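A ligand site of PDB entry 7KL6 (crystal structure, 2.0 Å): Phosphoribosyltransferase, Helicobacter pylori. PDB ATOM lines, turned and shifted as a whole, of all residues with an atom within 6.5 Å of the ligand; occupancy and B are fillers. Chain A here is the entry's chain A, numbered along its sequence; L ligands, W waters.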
ATOM      1  N   LEU A  75     -20.132  -1.508  -3.399  1.00  0.00           N
ATOM      2  CA  LEU A  75     -20.203  -0.473  -4.420  1.00  0.00           C
ATOM      3  C   LEU A  75     -20.027  -1.082  -5.804  1.00  0.00           C
ATOM      4  O   LEU A  75     -19.093  -1.851  -6.042  1.00  0.00           O
ATOM      5  CB  LEU A  75     -19.124   0.590  -4.173  1.00  0.00           C
ATOM      6  CG  LEU A  75     -19.002   1.742  -5.163  1.00  0.00           C
ATOM      7  CD1 LEU A  75     -20.260   2.597  -5.208  1.00  0.00           C
ATOM      8  CD2 LEU A  75     -17.773   2.592  -4.836  1.00  0.00           C
ATOM      9  N   ASP A  94     -20.697  15.511  -9.451  1.00  0.00           N
ATOM     10  CA  ASP A  94     -21.495  14.923  -8.383  1.00  0.00           C
ATOM     11  C   ASP A  94     -21.764  16.025  -7.366  1.00  0.00           C
ATOM     12  O   ASP A  94     -21.217  17.132  -7.492  1.00  0.00           O
ATOM     13  CB  ASP A  94     -20.770  13.720  -7.746  1.00  0.00           C
ATOM     14  CG  ASP A  94     -21.714  12.699  -7.177  1.00  0.00           C
ATOM     15  OD1 ASP A  94     -22.966  12.829  -7.322  1.00  0.00           O
ATOM     16  OD2 ASP A  94     -21.201  11.718  -6.603  1.00  0.00           O
ATOM     17  N   GLU A  95     -22.638  15.763  -6.392  1.00  0.00           N
ATOM     18  CA  GLU A  95     -23.060  16.876  -5.548  1.00  0.00           C
ATOM     19  C   GLU A  95     -22.245  16.940  -4.276  1.00  0.00           C
ATOM     20  O   GLU A  95     -21.943  18.033  -3.805  1.00  0.00           O
ATOM     21  CB  GLU A  95     -24.559  16.775  -5.168  1.00  0.00           C
ATOM     22  CG  GLU A  95     -24.971  15.952  -3.943  1.00  0.00           C
ATOM     23  CD  GLU A  95     -24.937  14.451  -4.067  1.00  0.00           C
ATOM     24  OE1 GLU A  95     -24.188  13.930  -4.929  1.00  0.00           O
ATOM     25  OE2 GLU A  95     -25.717  13.807  -3.338  1.00  0.00           O
ATOM     26  N   ILE A  96     -21.848  15.784  -3.724  1.00  0.00           N
ATOM     27  CA  ILE A  96     -21.067  15.759  -2.490  1.00  0.00           C
ATOM     28  C   ILE A  96     -20.053  14.614  -2.549  1.00  0.00           C
ATOM     29  O   ILE A  96     -20.355  13.525  -3.060  1.00  0.00           O
ATOM     30  CB  ILE A  96     -21.973  15.664  -1.236  1.00  0.00           C
ATOM     31  CG1 ILE A  96     -21.147  15.767   0.048  1.00  0.00           C
ATOM     32  CG2 ILE A  96     -22.814  14.395  -1.242  1.00  0.00           C
ATOM     33  CD1 ILE A  96     -21.990  15.948   1.353  1.00  0.00           C
ATOM     34  N   VAL A  97     -18.854  14.870  -2.060  1.00  0.00           N
ATOM     35  CA  VAL A  97     -17.841  13.831  -1.875  1.00  0.00           C
ATOM     36  C   VAL A  97     -17.775  13.555  -0.379  1.00  0.00           C
ATOM     37  O   VAL A  97     -17.406  14.443   0.397  1.00  0.00           O
ATOM     38  CB  VAL A  97     -16.471  14.248  -2.435  1.00  0.00           C
ATOM     39  CG1 VAL A  97     -15.386  13.245  -2.050  1.00  0.00           C
ATOM     40  CG2 VAL A  97     -16.537  14.377  -3.960  1.00  0.00           C
ATOM     41  N   ASP A  98     -18.134  12.336   0.005  1.00  0.00           N
ATOM     42  CA  ASP A  98     -18.170  11.962   1.422  1.00  0.00           C
ATOM     43  C   ASP A  98     -16.890  11.208   1.759  1.00  0.00           C
ATOM     44  O   ASP A  98     -15.925  11.807   2.238  1.00  0.00           O
ATOM     45  CB  ASP A  98     -19.423  11.120   1.714  1.00  0.00           C
ATOM     46  CG  ASP A  98     -19.720  11.000   3.206  1.00  0.00           C
ATOM     47  OD1 ASP A  98     -18.895  11.415   4.042  1.00  0.00           O
ATOM     48  OD2 ASP A  98     -20.788  10.457   3.547  1.00  0.00           O
ATOM     49  N   SER A  99     -16.880   9.895   1.510  1.00  0.00           N
ATOM     50  CA  SER A  99     -15.627   9.146   1.606  1.00  0.00           C
ATOM     51  C   SER A  99     -14.758   9.345   0.385  1.00  0.00           C
ATOM     52  O   SER A  99     -13.534   9.167   0.468  1.00  0.00           O
ATOM     53  CB  SER A  99     -15.890   7.654   1.789  1.00  0.00           C
ATOM     54  OG  SER A  99     -16.448   7.090   0.604  1.00  0.00           O
ATOM     55  N   GLY A 100     -15.350   9.739  -0.740  1.00  0.00           N
ATOM     56  CA  GLY A 100     -14.686   9.761  -2.026  1.00  0.00           C
ATOM     57  C   GLY A 100     -14.646   8.424  -2.749  1.00  0.00           C
ATOM     58  O   GLY A 100     -14.126   8.366  -3.874  1.00  0.00           O
ATOM     59  N   ASN A 101     -15.168   7.350  -2.135  1.00  0.00           N
ATOM     60  CA  ASN A 101     -15.022   6.019  -2.723  1.00  0.00           C
ATOM     61  C   ASN A 101     -15.755   5.912  -4.063  1.00  0.00           C
ATOM     62  O   ASN A 101     -15.239   5.304  -5.012  1.00  0.00           O
ATOM     63  CB  ASN A 101     -15.544   4.939  -1.764  1.00  0.00           C
ATOM     64  CG  ASN A 101     -14.583   4.635  -0.622  1.00  0.00           C
ATOM     65  OD1 ASN A 101     -13.360   4.707  -0.776  1.00  0.00           O
ATOM     66  ND2 ASN A 101     -15.133   4.282   0.518  1.00  0.00           N
ATOM     67  N   SER A 102     -16.954   6.478  -4.162  1.00  0.00           N
ATOM     68  CA  SER A 102     -17.720   6.299  -5.387  1.00  0.00           C
ATOM     69  C   SER A 102     -17.171   7.171  -6.516  1.00  0.00           C
ATOM     70  O   SER A 102     -17.065   6.721  -7.661  1.00  0.00           O
ATOM     71  CB  SER A 102     -19.217   6.573  -5.136  1.00  0.00           C
ATOM     72  OG  SER A 102     -19.452   7.878  -4.645  1.00  0.00           O
ATOM     73  N   LEU A 103     -16.755   8.410  -6.212  1.00  0.00           N
ATOM     74  CA  LEU A 103     -16.127   9.212  -7.262  1.00  0.00           C
ATOM     75  C   LEU A 103     -14.807   8.595  -7.718  1.00  0.00           C
ATOM     76  O   LEU A 103     -14.514   8.571  -8.921  1.00  0.00           O
ATOM     77  CB  LEU A 103     -15.931  10.651  -6.792  1.00  0.00           C
ATOM     78  CG  LEU A 103     -15.392  11.639  -7.827  1.00  0.00           C
ATOM     79  CD1 LEU A 103     -16.308  11.790  -9.029  1.00  0.00           C
ATOM     80  CD2 LEU A 103     -15.110  13.009  -7.198  1.00  0.00           C
ATOM     81  N   LYS A 127     -16.195  16.574   2.027  1.00  0.00           N
ATOM     82  CA  LYS A 127     -15.950  16.531   3.454  1.00  0.00           C
ATOM     83  C   LYS A 127     -14.441  16.406   3.592  1.00  0.00           C
ATOM     84  O   LYS A 127     -13.776  15.862   2.697  1.00  0.00           O
ATOM     85  CB  LYS A 127     -16.787  15.427   4.155  1.00  0.00           C
ATOM     86  CG  LYS A 127     -16.823  15.280   5.702  1.00  0.00           C
ATOM     87  CD  LYS A 127     -17.732  14.140   6.115  1.00  0.00           C
ATOM     88  CE  LYS A 127     -19.172  14.642   5.814  1.00  0.00           C
ATOM     89  NZ  LYS A 127     -19.584  15.841   6.729  1.00  0.00           N
ATOM     90  N   ALA A 141     -18.104  19.894   3.586  1.00  0.00           N
ATOM     91  CA  ALA A 141     -19.407  19.292   3.836  1.00  0.00           C
ATOM     92  C   ALA A 141     -19.717  19.347   5.324  1.00  0.00           C
ATOM     93  O   ALA A 141     -18.949  18.805   6.128  1.00  0.00           O
ATOM     94  CB  ALA A 141     -19.472  17.858   3.350  1.00  0.00           C
ATOM     95  N   PRO A 142     -20.822  19.974   5.733  1.00  0.00           N
ATOM     96  CA  PRO A 142     -21.191  19.979   7.158  1.00  0.00           C
ATOM     97  C   PRO A 142     -21.701  18.618   7.615  1.00  0.00           C
ATOM     98  O   PRO A 142     -21.853  17.711   6.797  1.00  0.00           O
ATOM     99  CB  PRO A 142     -22.294  21.043   7.229  1.00  0.00           C
ATOM    100  CG  PRO A 142     -22.899  21.037   5.866  1.00  0.00           C
ATOM    101  CD  PRO A 142     -21.778  20.721   4.896  1.00  0.00           C
ATOM    102  N   GLU A 143     -22.006  18.512   8.915  1.00  0.00           N
ATOM    103  CA  GLU A 143     -22.425  17.235   9.494  1.00  0.00           C
ATOM    104  C   GLU A 143     -23.576  16.604   8.705  1.00  0.00           C
ATOM    105  O   GLU A 143     -23.543  15.408   8.391  1.00  0.00           O
ATOM    106  CB  GLU A 143     -22.812  17.424  10.958  1.00  0.00           C
ATOM    107  N   TRP A 144     -24.603  17.391   8.379  1.00  0.00           N
ATOM    108  CA  TRP A 144     -25.600  16.888   7.428  1.00  0.00           C
ATOM    109  C   TRP A 144     -26.261  18.030   6.684  1.00  0.00           C
ATOM    110  O   TRP A 144     -26.491  19.116   7.226  1.00  0.00           O
ATOM    111  CB  TRP A 144     -26.665  16.006   8.092  1.00  0.00           C
ATOM    112  CG  TRP A 144     -27.448  15.205   7.060  1.00  0.00           C
ATOM    113  CD1 TRP A 144     -28.718  15.450   6.623  1.00  0.00           C
ATOM    114  CD2 TRP A 144     -26.985  14.074   6.308  1.00  0.00           C
ATOM    115  NE1 TRP A 144     -29.089  14.524   5.671  1.00  0.00           N
ATOM    116  CE2 TRP A 144     -28.037  13.672   5.457  1.00  0.00           C
ATOM    117  CE3 TRP A 144     -25.783  13.356   6.279  1.00  0.00           C
ATOM    118  CZ2 TRP A 144     -27.923  12.576   4.595  1.00  0.00           C
ATOM    119  CZ3 TRP A 144     -25.666  12.269   5.423  1.00  0.00           C
ATOM    120  CH2 TRP A 144     -26.737  11.896   4.593  1.00  0.00           C
ATOM    121  N   ILE A 145     -26.586  17.745   5.429  1.00  0.00           N
ATOM    122  CA  ILE A 145     -27.145  18.684   4.475  1.00  0.00           C
ATOM    123  C   ILE A 145     -28.341  18.038   3.780  1.00  0.00           C
ATOM    124  O   ILE A 145     -28.214  16.987   3.152  1.00  0.00           O
ATOM    125  CB  ILE A 145     -26.085  19.155   3.459  1.00  0.00           C
ATOM    126  CG1 ILE A 145     -26.593  20.343   2.651  1.00  0.00           C
ATOM    127  CG2 ILE A 145     -25.479  18.022   2.643  1.00  0.00           C
ATOM    128  CD1 ILE A 145     -25.627  20.785   1.632  1.00  0.00           C
ATOM    129  N   ASP A 146     -29.508  18.661   3.924  1.00  0.00           N
ATOM    130  CA  ASP A 146     -30.664  18.374   3.088  1.00  0.00           C
ATOM    131  C   ASP A 146     -30.521  19.143   1.783  1.00  0.00           C
ATOM    132  O   ASP A 146     -30.480  20.380   1.792  1.00  0.00           O
ATOM    133  CB  ASP A 146     -31.966  18.782   3.785  1.00  0.00           C
ATOM    134  CG  ASP A 146     -32.303  17.905   4.961  1.00  0.00           C
ATOM    135  OD1 ASP A 146     -33.385  18.093   5.556  1.00  0.00           O
ATOM    136  OD2 ASP A 146     -31.506  17.002   5.291  1.00  0.00           O
ATOM    137  N   PHE A 147     -30.475  18.442   0.658  1.00  0.00           N
ATOM    138  CA  PHE A 147     -30.453  19.113  -0.630  1.00  0.00           C
ATOM    139  C   PHE A 147     -31.876  19.359  -1.100  1.00  0.00           C
ATOM    140  O   PHE A 147     -32.756  18.521  -0.905  1.00  0.00           O
ATOM    141  CB  PHE A 147     -29.708  18.286  -1.670  1.00  0.00           C
ATOM    142  CG  PHE A 147     -28.224  18.206  -1.439  1.00  0.00           C
ATOM    143  CD1 PHE A 147     -27.680  17.215  -0.636  1.00  0.00           C
ATOM    144  CD2 PHE A 147     -27.373  19.127  -2.037  1.00  0.00           C
ATOM    145  CE1 PHE A 147     -26.306  17.141  -0.451  1.00  0.00           C
ATOM    146  CE2 PHE A 147     -26.010  19.064  -1.844  1.00  0.00           C
ATOM    147  CZ  PHE A 147     -25.473  18.079  -1.045  1.00  0.00           C
ATOM    148  N   GLU A 150     -33.728  16.721  -2.769  1.00  0.00           N
ATOM    149  CA  GLU A 150     -34.105  15.604  -1.899  1.00  0.00           C
ATOM    150  C   GLU A 150     -35.405  15.896  -1.129  1.00  0.00           C
ATOM    151  O   GLU A 150     -36.237  14.985  -0.944  1.00  0.00           O
ATOM    152  CB  GLU A 150     -32.983  15.361  -0.881  1.00  0.00           C
ATOM    153  CG  GLU A 150     -31.730  14.708  -1.415  1.00  0.00           C
ATOM    154  CD  GLU A 150     -30.573  14.662  -0.402  1.00  0.00           C
ATOM    155  OE1 GLU A 150     -30.605  15.397   0.634  1.00  0.00           O
ATOM    156  OE2 GLU A 150     -29.602  13.923  -0.681  1.00  0.00           O
HETATM  157  C1  LIG L   1     -20.944   8.888  -1.361  1.00  0.00           C
HETATM  158  C2  LIG L   1     -22.993  11.758   2.298  1.00  0.00           C
HETATM  159  C3  LIG L   1     -25.234  14.477   2.793  1.00  0.00           C
HETATM  160  C4  LIG L   1     -24.473  13.354   2.437  1.00  0.00           C
HETATM  161  C5  LIG L   1     -24.848  12.570   1.361  1.00  0.00           C
HETATM  162  C6  LIG L   1     -23.889  11.538   1.263  1.00  0.00           C
HETATM  163  C7  LIG L   1     -23.851  10.388   0.247  1.00  0.00           C
HETATM  164  C8  LIG L   1     -21.990  11.178  -1.008  1.00  0.00           C
HETATM  165  C9  LIG L   1     -21.161  10.301  -1.929  1.00  0.00           C
HETATM  166  C10 LIG L   1     -26.659  13.969   1.028  1.00  0.00           C
HETATM  167  N1  LIG L   1     -23.405  10.835  -1.060  1.00  0.00           N
HETATM  168  N2  LIG L   1     -23.357  12.837   2.967  1.00  0.00           N
HETATM  169  N3  LIG L   1     -25.951  12.903   0.671  1.00  0.00           N
HETATM  170  N4  LIG L   1     -26.318  14.731   2.062  1.00  0.00           N
HETATM  171  O1  LIG L   1     -24.864  15.287   3.887  1.00  0.00           O
HETATM  172  O2  LIG L   1     -18.311   9.781  -1.430  1.00  0.00           O
HETATM  173  O3  LIG L   1     -18.641   7.439  -1.989  1.00  0.00           O
HETATM  174  O4  LIG L   1     -18.869   8.148   0.326  1.00  0.00           O
HETATM  175  P1  LIG L   1     -19.138   8.548  -1.104  1.00  0.00           P
HETATM  176  O   HOH W   1     -17.476   9.840  -3.856  1.00  0.00           O
HETATM  177  O   HOH W   2     -22.887  11.316  -4.286  1.00  0.00           O
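An oxygen (O4) of the ligand sits at hydrogen-bond distance from the backbone NH of Ser 99, 2.9 Å away. OG of Ser 99 is in hydrogen-bond range of O4 of the ligand, at 2.7 Å. N of Ser 102 sits at hydrogen-bond distance from O3 of the ligand (2.9 Å). OG of Ser 102 lies within hydrogen-bond range of O3 of the ligand (2.8 Å). The backbone NH of Asp 98 lies within hydrogen-bond range of an oxygen (O2) of the ligand (2.9 Å). O2 of the ligand is in hydrogen-bond range of N of Gly 100, at 3.0 Å. The backbone NH of Ile 145 lies close to an oxygen (O1) of the ligand, at 3.4 Å. N4 of the ligand is in hydrogen-bond range of O of Ile 145. N of Asn 101 sits at hydrogen-bond distance from O3 of the ligand, at 3.5 Å.
The side-chain hydroxyl (OG) of Ser 99 sits at hydrogen-bond distance from the backbone NH (N) of Asn 101 (3.0 Å). The indole nitrogen (NE1) of Trp 144 sits close to the side-chain carboxylate (OD2) of Asp 146 (3.5 Å). The side-chain carboxylate (OE1) of Glu 150 sits at hydrogen-bond distance from the backbone NH (N) of Phe 147 (3.0 Å). O of Val 97 lies within hydrogen-bond range of N of Lys 127, 2.9 Å away.
CG2 of Ile 96 touches C8 of the ligand (3.3 Å). C of Val 97 touches O2 of the ligand, 3.95 Å away. CE3 of Trp 144 touches O1 of the ligand (3.2 Å). CE1 of Phe 147 touches N4 of the ligand (3.5 Å). Glu 150 touches the ligand. 11 residues have an atom within 4 Å of the ligand: Ile 96, Val 97, Asp 98, Ser 99, Gly 100, Asn 101, Ser 102, Trp 144, Ile 145, Phe 147 and Glu 150. The nearest printed residue that does not touch the ligand is Glu 95 (4.1 Å).
Water W1 lies within hydrogen-bond range of an oxygen (O2) of the ligand (2.6 Å), the backbone NH (N) of Leu 103 (2.8 Å) and the side-chain hydroxyl (OG) of Ser 102 (2.9 Å). Water W2 lies within hydrogen-bond range of OD2 of Asp 94, OE1 of Glu 95 and N1 of the ligand.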
